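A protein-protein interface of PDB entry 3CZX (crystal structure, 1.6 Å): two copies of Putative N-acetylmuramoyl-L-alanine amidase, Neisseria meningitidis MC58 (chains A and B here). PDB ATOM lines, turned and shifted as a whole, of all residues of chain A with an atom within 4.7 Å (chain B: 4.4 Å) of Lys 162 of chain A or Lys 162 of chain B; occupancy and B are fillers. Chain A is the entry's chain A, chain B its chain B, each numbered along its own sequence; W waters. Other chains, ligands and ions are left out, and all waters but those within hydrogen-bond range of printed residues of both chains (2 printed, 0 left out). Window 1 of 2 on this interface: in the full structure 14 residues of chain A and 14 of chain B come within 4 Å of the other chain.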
ATOM      1  N   ASP A  32      29.806  24.518  29.335  1.00  0.00           N
ATOM      2  CA  ASP A  32      28.470  24.542  29.933  1.00  0.00           C
ATOM      3  C   ASP A  32      28.567  24.085  31.384  1.00  0.00           C
ATOM      4  O   ASP A  32      27.967  24.697  32.283  1.00  0.00           O
ATOM      5  CB  ASP A  32      27.490  23.612  29.232  1.00  0.00           C
ATOM      6  CG  ASP A  32      26.900  24.213  27.957  1.00  0.00           C
ATOM      7  OD1 ASP A  32      27.123  25.425  27.722  1.00  0.00           O
ATOM      8  OD2 ASP A  32      26.247  23.431  27.219  1.00  0.00           O
ATOM      9  N   ILE A  36      27.537  26.689  34.358  1.00  0.00           N
ATOM     10  CA  ILE A  36      26.273  26.428  35.068  1.00  0.00           C
ATOM     11  C   ILE A  36      26.578  26.167  36.529  1.00  0.00           C
ATOM     12  O   ILE A  36      25.928  26.701  37.442  1.00  0.00           O
ATOM     13  CB  ILE A  36      25.477  25.302  34.453  1.00  0.00           C
ATOM     14  CG1 ILE A  36      25.084  25.686  33.011  1.00  0.00           C
ATOM     15  CG2 ILE A  36      24.255  24.994  35.266  1.00  0.00           C
ATOM     16  CD1 ILE A  36      24.504  24.517  32.255  1.00  0.00           C
ATOM     17  N   PHE A 158      22.550  13.506  29.175  1.00  0.00           N
ATOM     18  CA  PHE A 158      23.229  14.720  29.631  1.00  0.00           C
ATOM     19  C   PHE A 158      22.581  15.925  28.963  1.00  0.00           C
ATOM     20  O   PHE A 158      22.273  16.883  29.619  1.00  0.00           O
ATOM     21  CB  PHE A 158      24.715  14.746  29.357  1.00  0.00           C
ATOM     22  CG  PHE A 158      25.379  16.032  29.781  1.00  0.00           C
ATOM     23  CD1 PHE A 158      25.631  16.304  31.113  1.00  0.00           C
ATOM     24  CD2 PHE A 158      25.682  17.023  28.856  1.00  0.00           C
ATOM     25  CE1 PHE A 158      26.223  17.516  31.503  1.00  0.00           C
ATOM     26  CE2 PHE A 158      26.269  18.224  29.274  1.00  0.00           C
ATOM     27  CZ  PHE A 158      26.519  18.448  30.613  1.00  0.00           C
ATOM     28  N   LYS A 159      22.438  15.870  27.640  1.00  0.00           N
ATOM     29  CA  LYS A 159      21.913  17.025  26.911  1.00  0.00           C
ATOM     30  C   LYS A 159      20.512  17.423  27.354  1.00  0.00           C
ATOM     31  O   LYS A 159      20.196  18.614  27.356  1.00  0.00           O
ATOM     32  CB  LYS A 159      21.961  16.760  25.388  1.00  0.00           C
ATOM     33  CG  LYS A 159      23.345  16.700  24.812  1.00  0.00           C
ATOM     34  CD  LYS A 159      23.441  16.110  23.401  1.00  0.00           C
ATOM     35  CE  LYS A 159      22.895  16.971  22.360  1.00  0.00           C
ATOM     36  NZ  LYS A 159      23.137  16.373  20.985  1.00  0.00           N
ATOM     37  N   THR A 160      19.658  16.461  27.684  1.00  0.00           N
ATOM     38  CA  THR A 160      18.267  16.716  28.135  1.00  0.00           C
ATOM     39  C   THR A 160      18.131  17.083  29.600  1.00  0.00           C
ATOM     40  O   THR A 160      17.085  17.571  29.973  1.00  0.00           O
ATOM     41  CB  THR A 160      17.354  15.515  27.863  1.00  0.00           C
ATOM     42  OG1 THR A 160      17.776  14.406  28.677  1.00  0.00           O
ATOM     43  CG2 THR A 160      17.371  15.168  26.368  1.00  0.00           C
ATOM     44  N   THR A 161      19.179  16.855  30.410  1.00  0.00           N
ATOM     45  CA  THR A 161      19.126  17.083  31.873  1.00  0.00           C
ATOM     46  C   THR A 161      20.347  17.867  32.381  1.00  0.00           C
ATOM     47  O   THR A 161      20.630  17.869  33.549  1.00  0.00           O
ATOM     48  CB  THR A 161      18.993  15.760  32.635  1.00  0.00           C
ATOM     49  OG1 THR A 161      18.053  14.936  31.934  1.00  0.00           O
ATOM     50  CG2 THR A 161      18.474  15.974  34.062  1.00  0.00           C
ATOM     51  N   LYS A 162      20.987  18.586  31.486  1.00  0.00           N
ATOM     52  CA  LYS A 162      22.212  19.343  31.758  1.00  0.00           C
ATOM     53  C   LYS A 162      22.076  20.264  32.970  1.00  0.00           C
ATOM     54  O   LYS A 162      22.916  20.241  33.885  1.00  0.00           O
ATOM     55  CB  LYS A 162      22.493  20.188  30.499  1.00  0.00           C
ATOM     56  CG  LYS A 162      23.686  21.041  30.560  1.00  0.00           C
ATOM     57  CD  LYS A 162      24.046  21.482  29.181  1.00  0.00           C
ATOM     58  CE  LYS A 162      23.120  22.573  28.703  1.00  0.00           C
ATOM     59  NZ  LYS A 162      23.426  22.857  27.306  1.00  0.00           N
ATOM     60  N   TRP A 163      21.012  21.044  33.009  1.00  0.00           N
ATOM     61  CA  TRP A 163      20.893  22.040  34.076  1.00  0.00           C
ATOM     62  C   TRP A 163      20.644  21.368  35.400  1.00  0.00           C
ATOM     63  O   TRP A 163      21.141  21.810  36.441  1.00  0.00           O
ATOM     64  CB  TRP A 163      19.811  23.107  33.731  1.00  0.00           C
ATOM     65  CG  TRP A 163      20.205  23.946  32.591  1.00  0.00           C
ATOM     66  CD1 TRP A 163      20.103  23.639  31.269  1.00  0.00           C
ATOM     67  CD2 TRP A 163      20.808  25.242  32.649  1.00  0.00           C
ATOM     68  NE1 TRP A 163      20.624  24.644  30.500  1.00  0.00           N
ATOM     69  CE2 TRP A 163      21.066  25.642  31.320  1.00  0.00           C
ATOM     70  CE3 TRP A 163      21.173  26.099  33.697  1.00  0.00           C
ATOM     71  CZ2 TRP A 163      21.654  26.860  31.012  1.00  0.00           C
ATOM     72  CZ3 TRP A 163      21.769  27.304  33.376  1.00  0.00           C
ATOM     73  CH2 TRP A 163      22.002  27.671  32.051  1.00  0.00           C
ATOM     74  N   GLY A 164      19.887  20.273  35.380  1.00  0.00           N
ATOM     75  CA  GLY A 164      19.618  19.504  36.581  1.00  0.00           C
ATOM     76  C   GLY A 164      20.843  18.776  37.117  1.00  0.00           C
ATOM     77  O   GLY A 164      21.049  18.685  38.347  1.00  0.00           O
ATOM     78  N   ILE A 165      21.640  18.214  36.192  1.00  0.00           N
ATOM     79  CA  ILE A 165      22.883  17.539  36.567  1.00  0.00           C
ATOM     80  C   ILE A 165      23.853  18.558  37.199  1.00  0.00           C
ATOM     81  O   ILE A 165      24.441  18.293  38.257  1.00  0.00           O
ATOM     82  CB  ILE A 165      23.522  16.763  35.351  1.00  0.00           C
ATOM     83  CG1 ILE A 165      22.629  15.588  34.929  1.00  0.00           C
ATOM     84  CG2 ILE A 165      24.979  16.342  35.650  1.00  0.00           C
ATOM     85  CD1 ILE A 165      23.014  14.991  33.602  1.00  0.00           C
ATOM     86  N   CYS A 166      24.032  19.702  36.552  1.00  0.00           N
ATOM     87  CA  CYS A 166      24.948  20.752  37.043  1.00  0.00           C
ATOM     88  C   CYS A 166      24.440  21.348  38.345  1.00  0.00           C
ATOM     89  O   CYS A 166      25.242  21.615  39.231  1.00  0.00           O
ATOM     90  CB  CYS A 166      25.232  21.800  36.039  1.00  0.00           C
ATOM     91  SG  CYS A 166      26.060  21.187  34.547  1.00  0.00           S
ATOM     92  N   ASP B  32      18.379  26.853  27.292  1.00  0.00           N
ATOM     93  CA  ASP B  32      19.697  27.457  27.258  1.00  0.00           C
ATOM     94  C   ASP B  32      19.594  28.934  26.902  1.00  0.00           C
ATOM     95  O   ASP B  32      20.219  29.754  27.578  1.00  0.00           O
ATOM     96  CB  ASP B  32      20.637  26.767  26.235  1.00  0.00           C
ATOM     97  CG  ASP B  32      21.445  25.627  26.843  1.00  0.00           C
ATOM     98  OD1 ASP B  32      21.365  25.410  28.050  1.00  0.00           O
ATOM     99  OD2 ASP B  32      22.177  24.997  26.079  1.00  0.00           O
ATOM    100  N   ILE B  36      20.674  31.736  29.597  1.00  0.00           N
ATOM    101  CA  ILE B  36      21.919  32.463  29.359  1.00  0.00           C
ATOM    102  C   ILE B  36      21.655  33.941  29.154  1.00  0.00           C
ATOM    103  O   ILE B  36      22.314  34.780  29.751  1.00  0.00           O
ATOM    104  CB  ILE B  36      22.717  31.835  28.224  1.00  0.00           C
ATOM    105  CG1 ILE B  36      23.114  30.408  28.611  1.00  0.00           C
ATOM    106  CG2 ILE B  36      23.973  32.694  27.927  1.00  0.00           C
ATOM    107  CD1 ILE B  36      23.631  29.575  27.390  1.00  0.00           C
ATOM    108  N   PHE B 158      25.048  27.253  16.428  1.00  0.00           N
ATOM    109  CA  PHE B 158      24.483  27.668  17.714  1.00  0.00           C
ATOM    110  C   PHE B 158      25.229  26.966  18.824  1.00  0.00           C
ATOM    111  O   PHE B 158      25.564  27.579  19.832  1.00  0.00           O
ATOM    112  CB  PHE B 158      23.020  27.352  17.805  1.00  0.00           C
ATOM    113  CG  PHE B 158      22.441  27.653  19.156  1.00  0.00           C
ATOM    114  CD1 PHE B 158      22.144  28.950  19.521  1.00  0.00           C
ATOM    115  CD2 PHE B 158      22.237  26.645  20.062  1.00  0.00           C
ATOM    116  CE1 PHE B 158      21.610  29.221  20.818  1.00  0.00           C
ATOM    117  CE2 PHE B 158      21.747  26.917  21.347  1.00  0.00           C
ATOM    118  CZ  PHE B 158      21.416  28.195  21.698  1.00  0.00           C
ATOM    119  N   LYS B 159      25.397  25.656  18.672  1.00  0.00           N
ATOM    120  CA  LYS B 159      26.012  24.844  19.732  1.00  0.00           C
ATOM    121  C   LYS B 159      27.417  25.322  20.067  1.00  0.00           C
ATOM    122  O   LYS B 159      27.809  25.355  21.247  1.00  0.00           O
ATOM    123  CB  LYS B 159      25.988  23.364  19.361  1.00  0.00           C
ATOM    124  CG  LYS B 159      24.592  22.792  19.377  1.00  0.00           C
ATOM    125  CD  LYS B 159      24.476  21.434  18.710  1.00  0.00           C
ATOM    126  CE  LYS B 159      25.069  20.331  19.471  1.00  0.00           C
ATOM    127  NZ  LYS B 159      24.701  18.993  18.841  1.00  0.00           N
ATOM    128  N   THR B 160      28.191  25.734  19.051  1.00  0.00           N
ATOM    129  CA  THR B 160      29.582  26.138  19.280  1.00  0.00           C
ATOM    130  C   THR B 160      29.757  27.595  19.661  1.00  0.00           C
ATOM    131  O   THR B 160      30.809  27.968  20.202  1.00  0.00           O
ATOM    132  CB  THR B 160      30.500  25.795  18.066  1.00  0.00           C
ATOM    133  OG1 THR B 160      30.097  26.541  16.901  1.00  0.00           O
ATOM    134  CG2 THR B 160      30.420  24.310  17.758  1.00  0.00           C
ATOM    135  N   THR B 161      28.746  28.436  19.389  1.00  0.00           N
ATOM    136  CA  THR B 161      28.861  29.852  19.682  1.00  0.00           C
ATOM    137  C   THR B 161      27.742  30.422  20.526  1.00  0.00           C
ATOM    138  O   THR B 161      27.622  31.630  20.618  1.00  0.00           O
ATOM    139  CB  THR B 161      29.043  30.711  18.423  1.00  0.00           C
ATOM    140  OG1 THR B 161      27.861  30.729  17.626  1.00  0.00           O
ATOM    141  CG2 THR B 161      30.225  30.224  17.628  1.00  0.00           C
ATOM    142  N   LYS B 162      26.994  29.547  21.194  1.00  0.00           N
ATOM    143  CA  LYS B 162      25.782  29.997  21.881  1.00  0.00           C
ATOM    144  C   LYS B 162      26.018  31.074  22.921  1.00  0.00           C
ATOM    145  O   LYS B 162      25.217  31.979  23.038  1.00  0.00           O
ATOM    146  CB  LYS B 162      24.976  28.866  22.484  1.00  0.00           C
ATOM    147  CG  LYS B 162      25.615  28.106  23.536  1.00  0.00           C
ATOM    148  CD  LYS B 162      24.525  27.266  24.285  1.00  0.00           C
ATOM    149  CE  LYS B 162      25.096  26.587  25.512  1.00  0.00           C
ATOM    150  NZ  LYS B 162      25.614  25.260  25.239  1.00  0.00           N
ATOM    151  N   TRP B 163      27.120  30.988  23.661  1.00  0.00           N
ATOM    152  CA  TRP B 163      27.334  31.984  24.704  1.00  0.00           C
ATOM    153  C   TRP B 163      27.529  33.353  24.071  1.00  0.00           C
ATOM    154  O   TRP B 163      27.054  34.351  24.594  1.00  0.00           O
ATOM    155  CB  TRP B 163      28.437  31.585  25.685  1.00  0.00           C
ATOM    156  CG  TRP B 163      28.104  30.328  26.507  1.00  0.00           C
ATOM    157  CD1 TRP B 163      28.309  29.020  26.152  1.00  0.00           C
ATOM    158  CD2 TRP B 163      27.529  30.294  27.818  1.00  0.00           C
ATOM    159  NE1 TRP B 163      27.881  28.182  27.162  1.00  0.00           N
ATOM    160  CE2 TRP B 163      27.441  28.957  28.207  1.00  0.00           C
ATOM    161  CE3 TRP B 163      27.164  31.298  28.731  1.00  0.00           C
ATOM    162  CZ2 TRP B 163      26.885  28.572  29.448  1.00  0.00           C
ATOM    163  CZ3 TRP B 163      26.629  30.935  29.950  1.00  0.00           C
ATOM    164  CH2 TRP B 163      26.505  29.578  30.300  1.00  0.00           C
ATOM    165  N   GLY B 164      28.178  33.432  22.893  1.00  0.00           N
ATOM    166  CA  GLY B 164      28.331  34.673  22.146  1.00  0.00           C
ATOM    167  C   GLY B 164      27.026  35.167  21.505  1.00  0.00           C
ATOM    168  O   GLY B 164      26.735  36.357  21.474  1.00  0.00           O
ATOM    169  N   ILE B 165      26.233  34.241  20.976  1.00  0.00           N
ATOM    170  CA  ILE B 165      24.945  34.583  20.403  1.00  0.00           C
ATOM    171  C   ILE B 165      24.021  35.140  21.500  1.00  0.00           C
ATOM    172  O   ILE B 165      23.397  36.166  21.322  1.00  0.00           O
ATOM    173  CB  ILE B 165      24.250  33.371  19.702  1.00  0.00           C
ATOM    174  CG1 ILE B 165      25.097  32.923  18.486  1.00  0.00           C
ATOM    175  CG2 ILE B 165      22.844  33.744  19.298  1.00  0.00           C
ATOM    176  CD1 ILE B 165      24.582  31.562  17.880  1.00  0.00           C
ATOM    177  N   CYS B 166      24.013  34.488  22.658  1.00  0.00           N
ATOM    178  CA  CYS B 166      23.133  34.931  23.735  1.00  0.00           C
ATOM    179  C   CYS B 166      23.602  36.272  24.286  1.00  0.00           C
ATOM    180  O   CYS B 166      22.770  37.113  24.650  1.00  0.00           O
ATOM    181  CB  CYS B 166      23.063  33.886  24.832  1.00  0.00           C
ATOM    182  SG  CYS B 166      22.122  32.435  24.283  1.00  0.00           S
HETATM  183  O   HOH W   1      28.843  25.656  25.477  1.00  0.00           O
HETATM  184  O   HOH W   2      19.415  22.878  28.129  1.00  0.00           O
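The side-chain amino group (NZ) of Lys 162 of chain B lies within salt-bridge range of the side-chain carboxylate (OD2) of Asp 32 of chain A, at 2.8 Å.
The side-chain carboxylate (OD1) of Asp 32 of chain B sits at hydrogen-bond distance from the indole nitrogen (NE1) of Trp 163 of chain A, at 2.7 Å.
NZ of Lys 162 of chain A lies within salt-bridge range of OD2 of Asp 32 of chain B.
OD1 of Asp 32 of chain A is in hydrogen-bond range of NE1 of Trp 163 of chain B (2.9 Å).
The side-chain sulfur (SG) of Cys 166 of chain B is in hydrogen-bond range of the backbone carbonyl oxygen (O) of Lys 162 of chain B, 3.4 Å away.
The side-chain carboxylate (OD2) of Asp 32 of chain B lies within salt-bridge range of the side-chain amino group (NZ) of Lys 162 of chain B (3.5 Å).
The side-chain carboxylate of Asp 32 of chain A is in salt-bridge range of the side-chain amino group of Lys 162 of chain A (2.9 Å).
The backbone carbonyl oxygen (O) of Lys 162 of chain A lies within hydrogen-bond range of the side-chain sulfur (SG) of Cys 166 of chain A (3.3 Å).
Among the printed residues, merely in contact across the chains: Lys 159 of chain A with Lys 159 of chain B (3.7 Å) and Lys 162 of chain A with Lys 162 of chain B (3.9 Å).
Lys 162 of chain A touches just these residues of chain B: Asp 32 (2.8 Å) and Lys 162 (3.9 Å).
Printed residues of chain B within 4 Å of Trp 163 of chain A: Asp 32 (2.7 Å).
Lys 162 of chain B touches two residues of chain A.
Of the printed residues of chain A, Trp 163 of chain B touches Asp 32.
Ile 165 of chain B touches none of the printed residues of chain A.
Hydrophobic or aromatic side chains of chain B that line the printed part of chain A: Trp 163.
Along chain B the printed residues that touch a printed residue of chain A span positions 32 to 163.
Among the printed residues, 6 pairs touch across the chains.
Among the printed residues, Asp or Glu carboxylates within 4 Å of a Lys or Arg side-chain nitrogen of the other chain: Asp 32 of chain A with Lys 162 of chain B (2.8 Å) and Lys 162 of chain A with Asp 32 of chain B (2.8 Å).
Asp 32 of chain A touches Lys 162 of chain B, and with the chains exchanged Lys 162 of chain A touches Asp 32 of chain B.
Asp 32 of chain A touches Trp 163 of chain B, and with the chains exchanged Trp 163 of chain A touches Asp 32 of chain B.
Lys 159 of chain B touches its own counterpart, Lys 159 of chain A.
Lys 162 of chain B touches its own counterpart, Lys 162 of chain A.
11 positions are printed for both chains.
Of the 6 pairs that touch across the chains among the printed residues, 6 have their exchanged pair printed and touching as well.
Water W1 lies within hydrogen-bond range of the side-chain carboxylate (OD1) of Asp 32 of chain A (2.8 Å), the indole nitrogen (NE1) of Trp 163 of chain B (3.2 Å) and the side-chain amino group (NZ) of Lys 162 of chain B (3.3 Å).
Water W2 bridges the indole nitrogen of Trp 163 of chain A (3.2 Å) and the side-chain carboxylate of Asp 32 of chain B (3.2 Å).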
